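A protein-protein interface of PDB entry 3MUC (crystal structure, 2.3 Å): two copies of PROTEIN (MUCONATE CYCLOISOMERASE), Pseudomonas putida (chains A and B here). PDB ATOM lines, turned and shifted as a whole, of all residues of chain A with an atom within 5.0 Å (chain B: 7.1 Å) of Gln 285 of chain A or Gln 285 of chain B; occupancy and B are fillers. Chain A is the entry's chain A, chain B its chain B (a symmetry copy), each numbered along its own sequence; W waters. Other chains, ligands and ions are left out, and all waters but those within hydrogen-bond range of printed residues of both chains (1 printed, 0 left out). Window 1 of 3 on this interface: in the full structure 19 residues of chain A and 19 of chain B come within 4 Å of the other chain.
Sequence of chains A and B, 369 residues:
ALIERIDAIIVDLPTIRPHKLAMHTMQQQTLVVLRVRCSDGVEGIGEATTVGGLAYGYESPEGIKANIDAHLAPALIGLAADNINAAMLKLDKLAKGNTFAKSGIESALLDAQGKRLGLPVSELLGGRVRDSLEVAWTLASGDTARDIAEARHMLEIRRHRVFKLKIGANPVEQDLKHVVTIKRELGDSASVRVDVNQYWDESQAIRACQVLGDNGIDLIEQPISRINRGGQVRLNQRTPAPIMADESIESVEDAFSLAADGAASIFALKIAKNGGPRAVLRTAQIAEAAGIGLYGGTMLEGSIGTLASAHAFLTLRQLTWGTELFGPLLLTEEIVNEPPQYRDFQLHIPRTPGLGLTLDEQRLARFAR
The side-chain amide nitrogen (NE2) of Gln 285 of chain B sits close to the side-chain amide nitrogen (NE2) of Gln 285 of chain A.
The side-chain amide oxygen (OE1) of Gln 285 of chain A lies close to the backbone carbonyl oxygen (O) of Leu 281 of chain A. OE1 of Gln 285 of chain B sits close to O of Leu 281 of chain B, 3.1 Å away.
Among the printed residues, pairs that only touch across the chains: Arg 282 of chain A with Gln 285 of chain B (3.1 Å), Gln 285 of chain A with Arg 282 of chain B (3.1 Å), Ile 286 of chain A with Ala 289 of chain B (3.9 Å) and Ala 289 of chain A with Ile 286 of chain B (3.9 Å).
Gln 285 of chain B touches two residues of chain A. Printed residues of chain A within 4 Å of Ile 286 of chain B: Ala 289. Of the printed residues of chain B, Ile 286 of chain A touches Ala 289 (3.9 Å). Of the printed residues of chain A, Ala 289 of chain B touches Ile 286 (3.9 Å). Printed residues of chain B within 4 Å of Arg 282 of chain A: Gln 285 (3.1 Å). Of the printed residues of chain B, Ala 289 of chain A touches Ile 286 (3.9 Å). Val 252 of chain B touches none of the printed residues of chain A. The nearest residue of chain A that does not touch Gln 285 of chain B is Leu 281 of chain A (4.9 Å).
Of the 9 printed residues of chain A, 4 touch a printed residue of chain B. Hydrophobic or aromatic side chains of chain B that line the printed part of chain A: Ile 286 and Ala 289. Along chain B the printed residues that touch a printed residue of chain A span positions 282 to 289. Among the printed residues, no Asp or Glu carboxylate lies within 4 Å of a Lys or Arg side-chain nitrogen of the other chain.
Arg 282 of chain A touches Gln 285 of chain B, and with the chains exchanged Gln 285 of chain A touches Arg 282 of chain B. Gln 285 of chain B touches its own counterpart, Gln 285 of chain A. Ile 286 of chain A touches Ala 289 of chain B, and with the chains exchanged Ala 289 of chain A touches Ile 286 of chain B. Positions printed for both chains: 281, 282, 283, 284, 285, 286, 287, 288 and 289. Of the 5 pairs that touch across the chains among the printed residues, 5 have their exchanged pair printed and touching as well.
Water W1 lies within hydrogen-bond range of the backbone carbonyl oxygen (O) of Arg 282 of chain A (3.1 Å) and the side-chain amide nitrogen (NE2) of Gln 285 of chain B (3.3 Å).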
ATOM      1  N   LEU A 281     -14.302 -18.851   0.259  1.00  0.00           N
ATOM      2  CA  LEU A 281     -14.076 -17.708  -0.614  1.00  0.00           C
ATOM      3  C   LEU A 281     -12.820 -16.956  -0.200  1.00  0.00           C
ATOM      4  O   LEU A 281     -12.155 -16.358  -1.057  1.00  0.00           O
ATOM      5  CB  LEU A 281     -15.275 -16.761  -0.640  1.00  0.00           C
ATOM      6  CG  LEU A 281     -16.537 -17.288  -1.317  1.00  0.00           C
ATOM      7  CD1 LEU A 281     -17.506 -16.139  -1.482  1.00  0.00           C
ATOM      8  CD2 LEU A 281     -16.220 -17.902  -2.677  1.00  0.00           C
ATOM      9  N   ARG A 282     -12.480 -16.989   1.093  1.00  0.00           N
ATOM     10  CA  ARG A 282     -11.258 -16.329   1.573  1.00  0.00           C
ATOM     11  C   ARG A 282     -10.048 -17.071   0.991  1.00  0.00           C
ATOM     12  O   ARG A 282      -9.120 -16.455   0.457  1.00  0.00           O
ATOM     13  CB  ARG A 282     -11.167 -16.340   3.093  1.00  0.00           C
ATOM     14  CG  ARG A 282     -12.165 -15.457   3.777  1.00  0.00           C
ATOM     15  CD  ARG A 282     -11.989 -15.532   5.256  1.00  0.00           C
ATOM     16  NE  ARG A 282     -13.280 -15.469   5.933  1.00  0.00           N
ATOM     17  CZ  ARG A 282     -13.593 -16.171   7.018  1.00  0.00           C
ATOM     18  NH1 ARG A 282     -12.701 -16.994   7.566  1.00  0.00           N
ATOM     19  NH2 ARG A 282     -14.812 -16.075   7.533  1.00  0.00           N
ATOM     20  N   THR A 283     -10.106 -18.398   1.057  1.00  0.00           N
ATOM     21  CA  THR A 283      -9.055 -19.259   0.530  1.00  0.00           C
ATOM     22  C   THR A 283      -8.904 -19.051  -0.969  1.00  0.00           C
ATOM     23  O   THR A 283      -7.792 -18.948  -1.467  1.00  0.00           O
ATOM     24  CB  THR A 283      -9.348 -20.732   0.836  1.00  0.00           C
ATOM     25  OG1 THR A 283      -9.165 -20.947   2.238  1.00  0.00           O
ATOM     26  CG2 THR A 283      -8.428 -21.678   0.059  1.00  0.00           C
ATOM     27  N   ALA A 284     -10.030 -18.917  -1.665  1.00  0.00           N
ATOM     28  CA  ALA A 284     -10.020 -18.728  -3.107  1.00  0.00           C
ATOM     29  C   ALA A 284      -9.418 -17.382  -3.449  1.00  0.00           C
ATOM     30  O   ALA A 284      -8.698 -17.249  -4.441  1.00  0.00           O
ATOM     31  CB  ALA A 284     -11.422 -18.844  -3.670  1.00  0.00           C
ATOM     32  N   GLN A 285      -9.695 -16.392  -2.609  1.00  0.00           N
ATOM     33  CA  GLN A 285      -9.177 -15.040  -2.814  1.00  0.00           C
ATOM     34  C   GLN A 285      -7.665 -14.998  -2.659  1.00  0.00           C
ATOM     35  O   GLN A 285      -6.959 -14.346  -3.435  1.00  0.00           O
ATOM     36  CB  GLN A 285      -9.859 -14.054  -1.864  1.00  0.00           C
ATOM     37  CG  GLN A 285     -11.283 -13.737  -2.266  1.00  0.00           C
ATOM     38  CD  GLN A 285     -12.122 -13.152  -1.138  1.00  0.00           C
ATOM     39  OE1 GLN A 285     -13.318 -13.434  -1.042  1.00  0.00           O
ATOM     40  NE2 GLN A 285     -11.518 -12.311  -0.308  1.00  0.00           N
ATOM     41  N   ILE A 286      -7.162 -15.734  -1.682  1.00  0.00           N
ATOM     42  CA  ILE A 286      -5.727 -15.811  -1.436  1.00  0.00           C
ATOM     43  C   ILE A 286      -5.037 -16.437  -2.652  1.00  0.00           C
ATOM     44  O   ILE A 286      -4.011 -15.943  -3.125  1.00  0.00           O
ATOM     45  CB  ILE A 286      -5.437 -16.633  -0.139  1.00  0.00           C
ATOM     46  CG1 ILE A 286      -5.850 -15.811   1.072  1.00  0.00           C
ATOM     47  CG2 ILE A 286      -3.970 -17.033  -0.049  1.00  0.00           C
ATOM     48  CD1 ILE A 286      -5.765 -16.552   2.356  1.00  0.00           C
ATOM     49  N   ALA A 287      -5.635 -17.499  -3.181  1.00  0.00           N
ATOM     50  CA  ALA A 287      -5.076 -18.202  -4.336  1.00  0.00           C
ATOM     51  C   ALA A 287      -5.055 -17.291  -5.550  1.00  0.00           C
ATOM     52  O   ALA A 287      -4.074 -17.258  -6.298  1.00  0.00           O
ATOM     53  CB  ALA A 287      -5.888 -19.468  -4.636  1.00  0.00           C
ATOM     54  N   GLU A 288      -6.143 -16.545  -5.727  1.00  0.00           N
ATOM     55  CA  GLU A 288      -6.280 -15.606  -6.832  1.00  0.00           C
ATOM     56  C   GLU A 288      -5.216 -14.507  -6.795  1.00  0.00           C
ATOM     57  O   GLU A 288      -4.656 -14.146  -7.830  1.00  0.00           O
ATOM     58  CB  GLU A 288      -7.681 -14.992  -6.840  1.00  0.00           C
ATOM     59  CG  GLU A 288      -8.732 -15.798  -7.606  1.00  0.00           C
ATOM     60  CD  GLU A 288      -8.746 -15.505  -9.120  1.00  0.00           C
ATOM     61  OE1 GLU A 288      -8.912 -14.325  -9.497  1.00  0.00           O
ATOM     62  OE2 GLU A 288      -8.617 -16.456  -9.928  1.00  0.00           O
ATOM     63  N   ALA A 289      -4.914 -14.011  -5.602  1.00  0.00           N
ATOM     64  CA  ALA A 289      -3.921 -12.960  -5.424  1.00  0.00           C
ATOM     65  C   ALA A 289      -2.503 -13.473  -5.676  1.00  0.00           C
ATOM     66  O   ALA A 289      -1.584 -12.696  -5.906  1.00  0.00           O
ATOM     67  CB  ALA A 289      -4.027 -12.367  -4.032  1.00  0.00           C
ATOM     68  N   VAL B 252      -4.578  -5.562  -4.309  1.00  0.00           N
ATOM     69  CA  VAL B 252      -4.723  -6.670  -3.373  1.00  0.00           C
ATOM     70  C   VAL B 252      -3.525  -7.628  -3.518  1.00  0.00           C
ATOM     71  O   VAL B 252      -3.034  -8.184  -2.534  1.00  0.00           O
ATOM     72  CB  VAL B 252      -6.045  -7.444  -3.644  1.00  0.00           C
ATOM     73  CG1 VAL B 252      -6.112  -8.710  -2.824  1.00  0.00           C
ATOM     74  CG2 VAL B 252      -7.248  -6.568  -3.321  1.00  0.00           C
ATOM     75  N   PHE B 256      -0.553  -9.428  -0.815  1.00  0.00           N
ATOM     76  CA  PHE B 256      -0.110 -10.807  -0.702  1.00  0.00           C
ATOM     77  C   PHE B 256       1.425 -10.863  -0.729  1.00  0.00           C
ATOM     78  O   PHE B 256       2.059 -11.492   0.137  1.00  0.00           O
ATOM     79  CB  PHE B 256      -0.686 -11.664  -1.832  1.00  0.00           C
ATOM     80  CG  PHE B 256      -0.136 -13.070  -1.850  1.00  0.00           C
ATOM     81  CD1 PHE B 256      -0.574 -14.017  -0.921  1.00  0.00           C
ATOM     82  CD2 PHE B 256       0.901 -13.416  -2.704  1.00  0.00           C
ATOM     83  CE1 PHE B 256       0.034 -15.273  -0.845  1.00  0.00           C
ATOM     84  CE2 PHE B 256       1.503 -14.665  -2.622  1.00  0.00           C
ATOM     85  CZ  PHE B 256       1.071 -15.589  -1.692  1.00  0.00           C
ATOM     86  N   LEU B 269      -5.282   0.034   5.248  1.00  0.00           N
ATOM     87  CA  LEU B 269      -6.343  -0.384   4.337  1.00  0.00           C
ATOM     88  C   LEU B 269      -7.026   0.826   3.736  1.00  0.00           C
ATOM     89  O   LEU B 269      -7.614   1.624   4.459  1.00  0.00           O
ATOM     90  CB  LEU B 269      -7.388  -1.214   5.077  1.00  0.00           C
ATOM     91  CG  LEU B 269      -6.942  -2.438   5.868  1.00  0.00           C
ATOM     92  CD1 LEU B 269      -8.147  -3.018   6.532  1.00  0.00           C
ATOM     93  CD2 LEU B 269      -6.295  -3.467   4.966  1.00  0.00           C
ATOM     94  N   ARG B 278     -15.373  -3.962  -1.044  1.00  0.00           N
ATOM     95  CA  ARG B 278     -15.205  -5.422  -1.102  1.00  0.00           C
ATOM     96  C   ARG B 278     -13.735  -5.776  -1.336  1.00  0.00           C
ATOM     97  O   ARG B 278     -13.199  -6.719  -0.743  1.00  0.00           O
ATOM     98  CB  ARG B 278     -16.047  -6.029  -2.221  1.00  0.00           C
ATOM     99  CG  ARG B 278     -17.550  -5.833  -2.060  1.00  0.00           C
ATOM    100  CD  ARG B 278     -18.338  -6.163  -3.330  1.00  0.00           C
ATOM    101  NE  ARG B 278     -18.157  -7.546  -3.781  1.00  0.00           N
ATOM    102  CZ  ARG B 278     -17.569  -7.893  -4.922  1.00  0.00           C
ATOM    103  NH1 ARG B 278     -17.097  -6.962  -5.730  1.00  0.00           N
ATOM    104  NH2 ARG B 278     -17.461  -9.167  -5.263  1.00  0.00           N
ATOM    105  N   ALA B 279     -13.066  -4.990  -2.170  1.00  0.00           N
ATOM    106  CA  ALA B 279     -11.660  -5.228  -2.475  1.00  0.00           C
ATOM    107  C   ALA B 279     -10.778  -5.030  -1.242  1.00  0.00           C
ATOM    108  O   ALA B 279      -9.844  -5.808  -0.997  1.00  0.00           O
ATOM    109  CB  ALA B 279     -11.209  -4.335  -3.607  1.00  0.00           C
ATOM    110  N   VAL B 280     -11.093  -4.022  -0.439  1.00  0.00           N
ATOM    111  CA  VAL B 280     -10.296  -3.760   0.753  1.00  0.00           C
ATOM    112  C   VAL B 280     -10.440  -4.922   1.737  1.00  0.00           C
ATOM    113  O   VAL B 280      -9.527  -5.191   2.515  1.00  0.00           O
ATOM    114  CB  VAL B 280     -10.667  -2.404   1.404  1.00  0.00           C
ATOM    115  CG1 VAL B 280     -11.844  -2.549   2.369  1.00  0.00           C
ATOM    116  CG2 VAL B 280      -9.476  -1.826   2.098  1.00  0.00           C
ATOM    117  N   LEU B 281     -11.577  -5.624   1.675  1.00  0.00           N
ATOM    118  CA  LEU B 281     -11.819  -6.768   2.546  1.00  0.00           C
ATOM    119  C   LEU B 281     -10.958  -7.963   2.143  1.00  0.00           C
ATOM    120  O   LEU B 281     -10.572  -8.765   3.002  1.00  0.00           O
ATOM    121  CB  LEU B 281     -13.295  -7.156   2.585  1.00  0.00           C
ATOM    122  CG  LEU B 281     -14.246  -6.159   3.260  1.00  0.00           C
ATOM    123  CD1 LEU B 281     -15.590  -6.833   3.418  1.00  0.00           C
ATOM    124  CD2 LEU B 281     -13.709  -5.696   4.620  1.00  0.00           C
ATOM    125  N   ARG B 282     -10.651  -8.088   0.852  1.00  0.00           N
ATOM    126  CA  ARG B 282      -9.773  -9.164   0.379  1.00  0.00           C
ATOM    127  C   ARG B 282      -8.371  -8.934   0.950  1.00  0.00           C
ATOM    128  O   ARG B 282      -7.756  -9.856   1.491  1.00  0.00           O
ATOM    129  CB  ARG B 282      -9.681  -9.197  -1.136  1.00  0.00           C
ATOM    130  CG  ARG B 282     -10.954  -9.618  -1.826  1.00  0.00           C
ATOM    131  CD  ARG B 282     -10.775  -9.611  -3.311  1.00  0.00           C
ATOM    132  NE  ARG B 282     -11.991  -9.162  -3.985  1.00  0.00           N
ATOM    133  CZ  ARG B 282     -12.007  -8.372  -5.057  1.00  0.00           C
ATOM    134  NH1 ARG B 282     -10.869  -7.939  -5.597  1.00  0.00           N
ATOM    135  NH2 ARG B 282     -13.171  -7.999  -5.577  1.00  0.00           N
ATOM    136  N   THR B 283      -7.905  -7.686   0.877  1.00  0.00           N
ATOM    137  CA  THR B 283      -6.592  -7.306   1.400  1.00  0.00           C
ATOM    138  C   THR B 283      -6.510  -7.571   2.896  1.00  0.00           C
ATOM    139  O   THR B 283      -5.526  -8.115   3.384  1.00  0.00           O
ATOM    140  CB  THR B 283      -6.288  -5.822   1.101  1.00  0.00           C
ATOM    141  OG1 THR B 283      -6.018  -5.681  -0.298  1.00  0.00           O
ATOM    142  CG2 THR B 283      -5.076  -5.299   1.879  1.00  0.00           C
ATOM    143  N   ALA B 284      -7.586  -7.248   3.605  1.00  0.00           N
ATOM    144  CA  ALA B 284      -7.643  -7.433   5.041  1.00  0.00           C
ATOM    145  C   ALA B 284      -7.639  -8.905   5.376  1.00  0.00           C
ATOM    146  O   ALA B 284      -7.042  -9.317   6.367  1.00  0.00           O
ATOM    147  CB  ALA B 284      -8.880  -6.762   5.604  1.00  0.00           C
ATOM    148  N   GLN B 285      -8.297  -9.704   4.544  1.00  0.00           N
ATOM    149  CA  GLN B 285      -8.362 -11.152   4.766  1.00  0.00           C
ATOM    150  C   GLN B 285      -6.995 -11.779   4.602  1.00  0.00           C
ATOM    151  O   GLN B 285      -6.604 -12.658   5.382  1.00  0.00           O
ATOM    152  CB  GLN B 285      -9.381 -11.814   3.834  1.00  0.00           C
ATOM    153  CG  GLN B 285     -10.809 -11.555   4.243  1.00  0.00           C
ATOM    154  CD  GLN B 285     -11.807 -11.736   3.109  1.00  0.00           C
ATOM    155  OE1 GLN B 285     -12.767 -10.970   2.995  1.00  0.00           O
ATOM    156  NE2 GLN B 285     -11.613 -12.766   2.291  1.00  0.00           N
ATOM    157  N   ILE B 286      -6.241 -11.287   3.627  1.00  0.00           N
ATOM    158  CA  ILE B 286      -4.893 -11.784   3.370  1.00  0.00           C
ATOM    159  C   ILE B 286      -4.003 -11.481   4.580  1.00  0.00           C
ATOM    160  O   ILE B 286      -3.235 -12.335   5.035  1.00  0.00           O
ATOM    161  CB  ILE B 286      -4.312 -11.149   2.075  1.00  0.00           C
ATOM    162  CG1 ILE B 286      -5.017 -11.746   0.868  1.00  0.00           C
ATOM    163  CG2 ILE B 286      -2.805 -11.354   1.984  1.00  0.00           C
ATOM    164  CD1 ILE B 286      -4.664 -11.087  -0.415  1.00  0.00           C
ATOM    165  N   ALA B 287      -4.148 -10.274   5.122  1.00  0.00           N
ATOM    166  CA  ALA B 287      -3.344  -9.853   6.263  1.00  0.00           C
ATOM    167  C   ALA B 287      -3.666 -10.709   7.475  1.00  0.00           C
ATOM    168  O   ALA B 287      -2.765 -11.158   8.194  1.00  0.00           O
ATOM    169  CB  ALA B 287      -3.591  -8.378   6.568  1.00  0.00           C
ATOM    170  N   GLU B 288      -4.955 -10.966   7.664  1.00  0.00           N
ATOM    171  CA  GLU B 288      -5.446 -11.758   8.777  1.00  0.00           C
ATOM    172  C   GLU B 288      -4.904 -13.179   8.739  1.00  0.00           C
ATOM    173  O   GLU B 288      -4.539 -13.729   9.778  1.00  0.00           O
ATOM    174  CB  GLU B 288      -6.978 -11.770   8.789  1.00  0.00           C
ATOM    175  CG  GLU B 288      -7.625 -10.620   9.551  1.00  0.00           C
ATOM    176  CD  GLU B 288      -7.748 -10.889  11.056  1.00  0.00           C
ATOM    177  OE1 GLU B 288      -8.385 -11.902  11.431  1.00  0.00           O
ATOM    178  OE2 GLU B 288      -7.236 -10.074  11.862  1.00  0.00           O
ATOM    179  N   ALA B 289      -4.839 -13.759   7.544  1.00  0.00           N
ATOM    180  CA  ALA B 289      -4.346 -15.117   7.358  1.00  0.00           C
ATOM    181  C   ALA B 289      -2.848 -15.208   7.607  1.00  0.00           C
ATOM    182  O   ALA B 289      -2.326 -16.291   7.851  1.00  0.00           O
ATOM    183  CB  ALA B 289      -4.685 -15.622   5.962  1.00  0.00           C
ATOM    184  N   ALA B 290      -2.159 -14.072   7.543  1.00  0.00           N
ATOM    185  CA  ALA B 290      -0.716 -14.031   7.775  1.00  0.00           C
ATOM    186  C   ALA B 290      -0.353 -13.513   9.174  1.00  0.00           C
ATOM    187  O   ALA B 290       0.803 -13.600   9.572  1.00  0.00           O
ATOM    188  CB  ALA B 290      -0.037 -13.185   6.718  1.00  0.00           C
ATOM    189  N   GLY B 291      -1.318 -12.928   9.888  1.00  0.00           N
ATOM    190  CA  GLY B 291      -1.063 -12.408  11.226  1.00  0.00           C
ATOM    191  C   GLY B 291      -0.597 -10.959  11.250  1.00  0.00           C
ATOM    192  O   GLY B 291       0.045 -10.505  12.201  1.00  0.00           O
ATOM    193  N   LEU B 294      -3.965  -4.538  11.382  1.00  0.00           N
ATOM    194  CA  LEU B 294      -4.688  -3.619  10.505  1.00  0.00           C
ATOM    195  C   LEU B 294      -4.881  -2.193  11.012  1.00  0.00           C
ATOM    196  O   LEU B 294      -4.862  -1.918  12.223  1.00  0.00           O
ATOM    197  CB  LEU B 294      -6.040  -4.200  10.108  1.00  0.00           C
ATOM    198  CG  LEU B 294      -5.978  -5.589   9.458  1.00  0.00           C
ATOM    199  CD1 LEU B 294      -7.388  -6.121   9.238  1.00  0.00           C
ATOM    200  CD2 LEU B 294      -5.202  -5.527   8.151  1.00  0.00           C
ATOM    201  N   LEU B 316     -14.572  -6.072  10.204  1.00  0.00           N
ATOM    202  CA  LEU B 316     -13.292  -6.645  10.601  1.00  0.00           C
ATOM    203  C   LEU B 316     -13.225  -7.110  12.052  1.00  0.00           C
ATOM    204  O   LEU B 316     -13.643  -6.403  12.960  1.00  0.00           O
ATOM    205  CB  LEU B 316     -12.172  -5.641  10.324  1.00  0.00           C
ATOM    206  CG  LEU B 316     -11.359  -5.690   9.022  1.00  0.00           C
ATOM    207  CD1 LEU B 316     -12.029  -6.402   7.887  1.00  0.00           C
ATOM    208  CD2 LEU B 316     -11.042  -4.289   8.636  1.00  0.00           C
HETATM  209  O   HOH W   1      -8.687 -14.321   2.719  1.00  0.00           O
